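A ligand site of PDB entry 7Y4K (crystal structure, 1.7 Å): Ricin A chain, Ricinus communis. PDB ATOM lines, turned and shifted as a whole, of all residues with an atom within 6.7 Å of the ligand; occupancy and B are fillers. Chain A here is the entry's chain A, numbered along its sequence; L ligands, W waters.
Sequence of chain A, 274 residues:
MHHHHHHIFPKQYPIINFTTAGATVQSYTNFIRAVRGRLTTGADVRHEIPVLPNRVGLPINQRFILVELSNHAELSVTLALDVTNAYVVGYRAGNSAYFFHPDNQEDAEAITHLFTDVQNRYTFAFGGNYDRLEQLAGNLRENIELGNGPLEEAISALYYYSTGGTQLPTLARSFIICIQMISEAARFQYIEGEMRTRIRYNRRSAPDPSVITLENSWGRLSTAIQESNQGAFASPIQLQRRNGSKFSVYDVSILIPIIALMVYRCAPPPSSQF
Ala 86 touches the ligand. CE2 of Tyr 87 touches N3 of the ligand, 3.2 Å away. Phe 100 touches the ligand. Asn 129 touches the ligand. Ile 179 touches the ligand (CG2 to C2, 3.3 Å). Ser 183 touches the ligand (CB to O1, 3.4 Å). Glu 184 touches the ligand (OE2 to C6, 3.7 Å).
The backbone NH of Tyr 130 sits at hydrogen-bond distance from an oxygen (O2) of the ligand (2.8 Å). The guanidinium group of Arg 187 sits at hydrogen-bond distance from an oxygen (O1) of the ligand (2.8 Å). A nitrogen (N1) of the ligand sits at hydrogen-bond distance from the backbone carbonyl oxygen (O) of Val 88, 2.9 Å away. A nitrogen (N1) of the ligand lies within hydrogen-bond range of the backbone carbonyl oxygen (O) of Gly 128 (3.1 Å).
Water W2 lies within hydrogen-bond range of an oxygen (O2) of the ligand (2.9 Å), the backbone NH of Asp 131 (2.9 Å) and the backbone NH of Tyr 130 (3.4 Å).
The backbone carbonyl oxygen of Ala 86 is in hydrogen-bond range of the side-chain hydroxyl of Ser 183 (2.6 Å). OH of Tyr 130 is in hydrogen-bond range of OE2 of Glu 184. The backbone NH (N) of Tyr 87 lies close to the side-chain amide oxygen (OD1) of Asn 85, 3.1 Å away. N of Phe 100 sits at hydrogen-bond distance from O of Val 89, 3.1 Å away. The backbone carbonyl oxygen (O) of Asn 85 sits at hydrogen-bond distance from the guanidinium group (NH2) of Arg 187, at 2.7 Å. OH of Tyr 87 lies close to O of Gly 128, at 3.4 Å. The backbone NH (N) of Glu 184 is in hydrogen-bond range of the backbone carbonyl oxygen (O) of Ile 179. The side-chain amide oxygen (OD1) of Asn 129 lies within hydrogen-bond range of the side-chain hydroxyl (OH) of Tyr 87.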
ATOM      1  N   LEU A  81     -10.545   0.939 -21.742  1.00  0.00           N
ATOM      2  CA  LEU A  81     -10.742   2.302 -22.231  1.00  0.00           C
ATOM      3  C   LEU A  81      -9.897   2.557 -23.468  1.00  0.00           C
ATOM      4  O   LEU A  81      -8.721   2.208 -23.513  1.00  0.00           O
ATOM      5  CB  LEU A  81     -10.418   3.338 -21.143  1.00  0.00           C
ATOM      6  CG  LEU A  81     -11.486   3.690 -20.089  1.00  0.00           C
ATOM      7  CD1 LEU A  81     -11.753   2.530 -19.124  1.00  0.00           C
ATOM      8  CD2 LEU A  81     -11.047   4.919 -19.314  1.00  0.00           C
ATOM      9  N   ASN A  85     -10.279   8.535 -26.889  1.00  0.00           N
ATOM     10  CA  ASN A  85     -11.464   9.261 -26.416  1.00  0.00           C
ATOM     11  C   ASN A  85     -11.859   8.983 -24.953  1.00  0.00           C
ATOM     12  O   ASN A  85     -12.867   9.528 -24.473  1.00  0.00           O
ATOM     13  CB  ASN A  85     -12.651   9.037 -27.357  1.00  0.00           C
ATOM     14  CG  ASN A  85     -12.921   7.554 -27.610  1.00  0.00           C
ATOM     15  OD1 ASN A  85     -12.424   6.683 -26.898  1.00  0.00           O
ATOM     16  ND2 ASN A  85     -13.724   7.276 -28.630  1.00  0.00           N
ATOM     17  N   ALA A  86     -11.056   8.155 -24.275  1.00  0.00           N
ATOM     18  CA  ALA A  86     -11.335   7.667 -22.903  1.00  0.00           C
ATOM     19  C   ALA A  86     -12.643   6.858 -22.781  1.00  0.00           C
ATOM     20  O   ALA A  86     -13.133   6.629 -21.675  1.00  0.00           O
ATOM     21  CB  ALA A  86     -11.279   8.815 -21.884  1.00  0.00           C
ATOM     22  N   TYR A  87     -13.180   6.405 -23.915  1.00  0.00           N
ATOM     23  CA  TYR A  87     -14.424   5.635 -23.990  1.00  0.00           C
ATOM     24  C   TYR A  87     -14.254   4.250 -23.367  1.00  0.00           C
ATOM     25  O   TYR A  87     -13.250   3.560 -23.638  1.00  0.00           O
ATOM     26  CB  TYR A  87     -14.780   5.497 -25.464  1.00  0.00           C
ATOM     27  CG  TYR A  87     -16.191   5.161 -25.800  1.00  0.00           C
ATOM     28  CD1 TYR A  87     -16.596   3.845 -25.940  1.00  0.00           C
ATOM     29  CD2 TYR A  87     -17.120   6.161 -26.036  1.00  0.00           C
ATOM     30  CE1 TYR A  87     -17.891   3.529 -26.270  1.00  0.00           C
ATOM     31  CE2 TYR A  87     -18.420   5.856 -26.378  1.00  0.00           C
ATOM     32  CZ  TYR A  87     -18.796   4.544 -26.482  1.00  0.00           C
ATOM     33  OH  TYR A  87     -20.088   4.233 -26.824  1.00  0.00           O
ATOM     34  N   VAL A  88     -15.216   3.833 -22.540  1.00  0.00           N
ATOM     35  CA  VAL A  88     -15.262   2.462 -22.037  1.00  0.00           C
ATOM     36  C   VAL A  88     -15.817   1.619 -23.177  1.00  0.00           C
ATOM     37  O   VAL A  88     -16.984   1.775 -23.550  1.00  0.00           O
ATOM     38  CB  VAL A  88     -16.158   2.340 -20.788  1.00  0.00           C
ATOM     39  CG1 VAL A  88     -16.211   0.893 -20.298  1.00  0.00           C
ATOM     40  CG2 VAL A  88     -15.670   3.260 -19.683  1.00  0.00           C
ATOM     41  N   VAL A  89     -14.977   0.753 -23.744  1.00  0.00           N
ATOM     42  CA  VAL A  89     -15.376  -0.048 -24.912  1.00  0.00           C
ATOM     43  C   VAL A  89     -15.912  -1.434 -24.534  1.00  0.00           C
ATOM     44  O   VAL A  89     -16.571  -2.107 -25.339  1.00  0.00           O
ATOM     45  CB  VAL A  89     -14.250  -0.173 -25.972  1.00  0.00           C
ATOM     46  CG1 VAL A  89     -13.818   1.211 -26.465  1.00  0.00           C
ATOM     47  CG2 VAL A  89     -13.054  -0.974 -25.455  1.00  0.00           C
ATOM     48  N   GLY A  90     -15.627  -1.850 -23.311  1.00  0.00           N
ATOM     49  CA  GLY A  90     -16.077  -3.142 -22.814  1.00  0.00           C
ATOM     50  C   GLY A  90     -15.506  -3.464 -21.455  1.00  0.00           C
ATOM     51  O   GLY A  90     -14.776  -2.658 -20.858  1.00  0.00           O
ATOM     52  N   PHE A 100     -19.250  -3.301 -26.194  1.00  0.00           N
ATOM     53  CA  PHE A 100     -20.313  -2.551 -26.870  1.00  0.00           C
ATOM     54  C   PHE A 100     -20.175  -2.746 -28.381  1.00  0.00           C
ATOM     55  O   PHE A 100     -19.067  -3.009 -28.878  1.00  0.00           O
ATOM     56  CB  PHE A 100     -20.263  -1.063 -26.516  1.00  0.00           C
ATOM     57  CG  PHE A 100     -20.525  -0.781 -25.054  1.00  0.00           C
ATOM     58  CD1 PHE A 100     -21.766  -1.080 -24.483  1.00  0.00           C
ATOM     59  CD2 PHE A 100     -19.531  -0.196 -24.270  1.00  0.00           C
ATOM     60  CE1 PHE A 100     -22.005  -0.799 -23.129  1.00  0.00           C
ATOM     61  CE2 PHE A 100     -19.771   0.069 -22.923  1.00  0.00           C
ATOM     62  CZ  PHE A 100     -21.004  -0.236 -22.352  1.00  0.00           C
ATOM     63  N   GLY A 127     -24.830  -0.188 -28.880  1.00  0.00           N
ATOM     64  CA  GLY A 127     -23.673   0.696 -28.669  1.00  0.00           C
ATOM     65  C   GLY A 127     -23.632   1.164 -27.219  1.00  0.00           C
ATOM     66  O   GLY A 127     -24.606   0.983 -26.483  1.00  0.00           O
ATOM     67  N   GLY A 128     -22.521   1.782 -26.827  1.00  0.00           N
ATOM     68  CA  GLY A 128     -22.317   2.219 -25.452  1.00  0.00           C
ATOM     69  C   GLY A 128     -22.486   3.682 -25.116  1.00  0.00           C
ATOM     70  O   GLY A 128     -22.063   4.118 -24.050  1.00  0.00           O
ATOM     71  N   ASN A 129     -23.100   4.452 -26.034  1.00  0.00           N
ATOM     72  CA  ASN A 129     -23.366   5.872 -25.805  1.00  0.00           C
ATOM     73  C   ASN A 129     -24.441   6.081 -24.730  1.00  0.00           C
ATOM     74  O   ASN A 129     -25.249   5.168 -24.469  1.00  0.00           O
ATOM     75  CB  ASN A 129     -23.755   6.585 -27.105  1.00  0.00           C
ATOM     76  CG  ASN A 129     -22.591   6.708 -28.081  1.00  0.00           C
ATOM     77  OD1 ASN A 129     -21.467   6.331 -27.767  1.00  0.00           O
ATOM     78  ND2 ASN A 129     -22.875   7.241 -29.268  1.00  0.00           N
ATOM     79  N   TYR A 130     -24.434   7.256 -24.103  1.00  0.00           N
ATOM     80  CA  TYR A 130     -25.415   7.573 -23.038  1.00  0.00           C
ATOM     81  C   TYR A 130     -26.861   7.410 -23.509  1.00  0.00           C
ATOM     82  O   TYR A 130     -27.670   6.816 -22.786  1.00  0.00           O
ATOM     83  CB  TYR A 130     -25.236   8.995 -22.485  1.00  0.00           C
ATOM     84  CG  TYR A 130     -24.008   9.209 -21.632  1.00  0.00           C
ATOM     85  CD1 TYR A 130     -23.595   8.271 -20.662  1.00  0.00           C
ATOM     86  CD2 TYR A 130     -23.270  10.393 -21.753  1.00  0.00           C
ATOM     87  CE1 TYR A 130     -22.472   8.497 -19.886  1.00  0.00           C
ATOM     88  CE2 TYR A 130     -22.149  10.632 -20.980  1.00  0.00           C
ATOM     89  CZ  TYR A 130     -21.750   9.676 -20.054  1.00  0.00           C
ATOM     90  OH  TYR A 130     -20.651   9.920 -19.278  1.00  0.00           O
ATOM     91  N   ASP A 131     -27.174   7.906 -24.713  1.00  0.00           N
ATOM     92  CA  ASP A 131     -28.520   7.794 -25.307  1.00  0.00           C
ATOM     93  C   ASP A 131     -29.048   6.359 -25.232  1.00  0.00           C
ATOM     94  O   ASP A 131     -30.144   6.120 -24.701  1.00  0.00           O
ATOM     95  CB  ASP A 131     -28.537   8.306 -26.756  1.00  0.00           C
ATOM     96  CG  ASP A 131     -28.660   9.825 -26.865  1.00  0.00           C
ATOM     97  OD1 ASP A 131     -28.846  10.517 -25.849  1.00  0.00           O
ATOM     98  OD2 ASP A 131     -28.569  10.339 -28.012  1.00  0.00           O
ATOM     99  N   LEU A 133     -27.688   3.767 -23.493  1.00  0.00           N
ATOM    100  CA  LEU A 133     -27.606   3.210 -22.140  1.00  0.00           C
ATOM    101  C   LEU A 133     -28.757   3.672 -21.241  1.00  0.00           C
ATOM    102  O   LEU A 133     -29.293   2.875 -20.482  1.00  0.00           O
ATOM    103  CB  LEU A 133     -26.240   3.479 -21.501  1.00  0.00           C
ATOM    104  CG  LEU A 133     -25.019   2.722 -22.057  1.00  0.00           C
ATOM    105  CD1 LEU A 133     -23.783   3.181 -21.300  1.00  0.00           C
ATOM    106  CD2 LEU A 133     -25.138   1.197 -21.964  1.00  0.00           C
ATOM    107  N   ARG A 141     -29.375  10.050 -17.036  1.00  0.00           N
ATOM    108  CA  ARG A 141     -28.264  10.406 -16.141  1.00  0.00           C
ATOM    109  C   ARG A 141     -28.703  11.291 -14.964  1.00  0.00           C
ATOM    110  O   ARG A 141     -28.266  11.063 -13.841  1.00  0.00           O
ATOM    111  CB  ARG A 141     -27.144  11.082 -16.927  1.00  0.00           C
ATOM    112  CG  ARG A 141     -26.228  10.138 -17.668  1.00  0.00           C
ATOM    113  CD  ARG A 141     -25.356  10.954 -18.617  1.00  0.00           C
ATOM    114  NE  ARG A 141     -26.089  11.406 -19.808  1.00  0.00           N
ATOM    115  CZ  ARG A 141     -25.736  12.425 -20.582  1.00  0.00           C
ATOM    116  NH1 ARG A 141     -24.657  13.154 -20.313  1.00  0.00           N
ATOM    117  NH2 ARG A 141     -26.476  12.716 -21.654  1.00  0.00           N
ATOM    118  N   PHE A 175     -23.103   0.713 -16.014  1.00  0.00           N
ATOM    119  CA  PHE A 175     -22.189   1.302 -17.004  1.00  0.00           C
ATOM    120  C   PHE A 175     -22.193   2.825 -16.887  1.00  0.00           C
ATOM    121  O   PHE A 175     -21.124   3.445 -16.873  1.00  0.00           O
ATOM    122  CB  PHE A 175     -22.555   0.901 -18.440  1.00  0.00           C
ATOM    123  CG  PHE A 175     -22.112  -0.480 -18.845  1.00  0.00           C
ATOM    124  CD1 PHE A 175     -20.807  -0.930 -18.610  1.00  0.00           C
ATOM    125  CD2 PHE A 175     -22.995  -1.321 -19.531  1.00  0.00           C
ATOM    126  CE1 PHE A 175     -20.412  -2.208 -19.007  1.00  0.00           C
ATOM    127  CE2 PHE A 175     -22.608  -2.593 -19.928  1.00  0.00           C
ATOM    128  CZ  PHE A 175     -21.321  -3.034 -19.671  1.00  0.00           C
ATOM    129  N   ILE A 179     -18.812   4.973 -16.252  1.00  0.00           N
ATOM    130  CA  ILE A 179     -18.388   5.926 -17.284  1.00  0.00           C
ATOM    131  C   ILE A 179     -18.195   7.333 -16.710  1.00  0.00           C
ATOM    132  O   ILE A 179     -17.186   7.982 -16.962  1.00  0.00           O
ATOM    133  CB  ILE A 179     -19.355   5.936 -18.493  1.00  0.00           C
ATOM    134  CG1 ILE A 179     -19.281   4.587 -19.222  1.00  0.00           C
ATOM    135  CG2 ILE A 179     -19.032   7.069 -19.452  1.00  0.00           C
ATOM    136  CD1 ILE A 179     -20.524   4.288 -20.054  1.00  0.00           C
ATOM    137  N   GLN A 180     -19.152   7.789 -15.897  1.00  0.00           N
ATOM    138  CA  GLN A 180     -19.067   9.136 -15.353  1.00  0.00           C
ATOM    139  C   GLN A 180     -17.988   9.279 -14.281  1.00  0.00           C
ATOM    140  O   GLN A 180     -17.282  10.283 -14.243  1.00  0.00           O
ATOM    141  CB  GLN A 180     -20.430   9.590 -14.819  1.00  0.00           C
ATOM    142  CG  GLN A 180     -21.427   9.756 -15.942  1.00  0.00           C
ATOM    143  CD  GLN A 180     -22.781  10.123 -15.412  1.00  0.00           C
ATOM    144  OE1 GLN A 180     -23.588   9.259 -15.088  1.00  0.00           O
ATOM    145  NE2 GLN A 180     -23.021  11.414 -15.275  1.00  0.00           N
ATOM    146  N   SER A 183     -14.321   7.826 -16.783  1.00  0.00           N
ATOM    147  CA  SER A 183     -14.029   8.543 -18.031  1.00  0.00           C
ATOM    148  C   SER A 183     -14.308  10.049 -17.954  1.00  0.00           C
ATOM    149  O   SER A 183     -13.461  10.868 -18.327  1.00  0.00           O
ATOM    150  CB  SER A 183     -14.777   7.910 -19.202  1.00  0.00           C
ATOM    151  OG  SER A 183     -14.394   6.560 -19.353  1.00  0.00           O
ATOM    152  N   GLU A 184     -15.497  10.421 -17.465  1.00  0.00           N
ATOM    153  CA  GLU A 184     -15.837  11.846 -17.380  1.00  0.00           C
ATOM    154  C   GLU A 184     -14.975  12.584 -16.366  1.00  0.00           C
ATOM    155  O   GLU A 184     -14.557  13.711 -16.625  1.00  0.00           O
ATOM    156  CB  GLU A 184     -17.323  12.076 -17.077  1.00  0.00           C
ATOM    157  CG  GLU A 184     -18.270  11.475 -18.104  1.00  0.00           C
ATOM    158  CD  GLU A 184     -18.254  12.145 -19.479  1.00  0.00           C
ATOM    159  OE1 GLU A 184     -17.390  13.001 -19.780  1.00  0.00           O
ATOM    160  OE2 GLU A 184     -19.136  11.791 -20.292  1.00  0.00           O
ATOM    161  N   ARG A 187     -11.713  13.216 -18.042  1.00  0.00           N
ATOM    162  CA  ARG A 187     -11.867  14.316 -19.001  1.00  0.00           C
ATOM    163  C   ARG A 187     -11.979  15.699 -18.366  1.00  0.00           C
ATOM    164  O   ARG A 187     -11.456  16.672 -18.911  1.00  0.00           O
ATOM    165  CB  ARG A 187     -13.091  14.091 -19.873  1.00  0.00           C
ATOM    166  CG  ARG A 187     -12.992  12.898 -20.806  1.00  0.00           C
ATOM    167  CD  ARG A 187     -14.331  12.683 -21.493  1.00  0.00           C
ATOM    168  NE  ARG A 187     -14.311  11.432 -22.275  1.00  0.00           N
ATOM    169  CZ  ARG A 187     -15.255  10.492 -22.232  1.00  0.00           C
ATOM    170  NH1 ARG A 187     -16.325  10.615 -21.462  1.00  0.00           N
ATOM    171  NH2 ARG A 187     -15.117   9.413 -22.979  1.00  0.00           N
ATOM    172  N   GLU A 215     -20.561  16.955 -19.875  1.00  0.00           N
ATOM    173  CA  GLU A 215     -20.467  15.633 -20.520  1.00  0.00           C
ATOM    174  C   GLU A 215     -20.969  15.699 -21.950  1.00  0.00           C
ATOM    175  O   GLU A 215     -20.322  15.201 -22.874  1.00  0.00           O
ATOM    176  CB  GLU A 215     -21.248  14.577 -19.765  1.00  0.00           C
ATOM    177  CG  GLU A 215     -20.773  14.325 -18.331  1.00  0.00           C
ATOM    178  CD  GLU A 215     -21.698  13.427 -17.542  1.00  0.00           C
ATOM    179  OE1 GLU A 215     -22.800  13.089 -18.038  1.00  0.00           O
ATOM    180  OE2 GLU A 215     -21.321  13.035 -16.424  1.00  0.00           O
ATOM    181  N   ASN A 216     -22.117  16.357 -22.144  1.00  0.00           N
ATOM    182  CA  ASN A 216     -22.717  16.490 -23.478  1.00  0.00           C
ATOM    183  C   ASN A 216     -21.904  17.345 -24.445  1.00  0.00           C
ATOM    184  O   ASN A 216     -21.991  17.176 -25.660  1.00  0.00           O
ATOM    185  CB  ASN A 216     -24.144  17.021 -23.375  1.00  0.00           C
ATOM    186  CG  ASN A 216     -25.085  16.020 -22.727  1.00  0.00           C
ATOM    187  OD1 ASN A 216     -24.810  14.822 -22.673  1.00  0.00           O
ATOM    188  ND2 ASN A 216     -26.206  16.514 -22.226  1.00  0.00           N
ATOM    189  N   TRP A 218     -18.420  17.782 -24.435  1.00  0.00           N
ATOM    190  CA  TRP A 218     -16.974  17.476 -24.485  1.00  0.00           C
ATOM    191  C   TRP A 218     -16.385  17.578 -25.893  1.00  0.00           C
ATOM    192  O   TRP A 218     -15.358  18.231 -26.096  1.00  0.00           O
ATOM    193  CB  TRP A 218     -16.663  16.128 -23.865  1.00  0.00           C
ATOM    194  CG  TRP A 218     -15.175  15.841 -23.771  1.00  0.00           C
ATOM    195  CD1 TRP A 218     -14.228  16.601 -23.142  1.00  0.00           C
ATOM    196  CD2 TRP A 218     -14.475  14.706 -24.296  1.00  0.00           C
ATOM    197  NE1 TRP A 218     -12.983  16.013 -23.240  1.00  0.00           N
ATOM    198  CE2 TRP A 218     -13.110  14.847 -23.951  1.00  0.00           C
ATOM    199  CE3 TRP A 218     -14.869  13.568 -25.048  1.00  0.00           C
ATOM    200  CZ2 TRP A 218     -12.129  13.897 -24.308  1.00  0.00           C
ATOM    201  CZ3 TRP A 218     -13.887  12.619 -25.405  1.00  0.00           C
ATOM    202  CH2 TRP A 218     -12.531  12.800 -25.036  1.00  0.00           C
HETATM  203  C1  LIG L   1     -19.010   4.925 -23.096  1.00  0.00           C
HETATM  204  N1  LIG L   1     -19.167   3.604 -23.166  1.00  0.00           N
HETATM  205  O1  LIG L   1     -16.657   7.293 -21.990  1.00  0.00           O
HETATM  206  C2  LIG L   1     -17.682   6.842 -22.496  1.00  0.00           C
HETATM  207  N2  LIG L   1     -17.841   5.451 -22.550  1.00  0.00           N
HETATM  208  C3  LIG L   1     -18.699   7.680 -22.971  1.00  0.00           C
HETATM  209  N3  LIG L   1     -19.973   5.753 -23.558  1.00  0.00           N
HETATM  210  O2  LIG L   1     -22.842   9.409 -24.963  1.00  0.00           O
HETATM  211  C4  LIG L   1     -19.853   7.091 -23.517  1.00  0.00           C
HETATM  212  N4  LIG L   1     -20.850   7.859 -24.002  1.00  0.00           N
HETATM  213  C5  LIG L   1     -20.773   9.207 -23.986  1.00  0.00           C
HETATM  214  N5  LIG L   1     -18.593   9.017 -22.927  1.00  0.00           N
HETATM  215  C6  LIG L   1     -19.627   9.818 -23.433  1.00  0.00           C
HETATM  216  C7  LIG L   1     -21.823   9.955 -24.529  1.00  0.00           C
HETATM  217  N6  LIG L   1     -21.603  11.265 -24.687  1.00  0.00           N
HETATM  218  O   HOH W   1     -18.458  12.335 -25.439  1.00  0.00           O
HETATM  219  O   HOH W   2     -25.398   9.669 -26.250  1.00  0.00           O
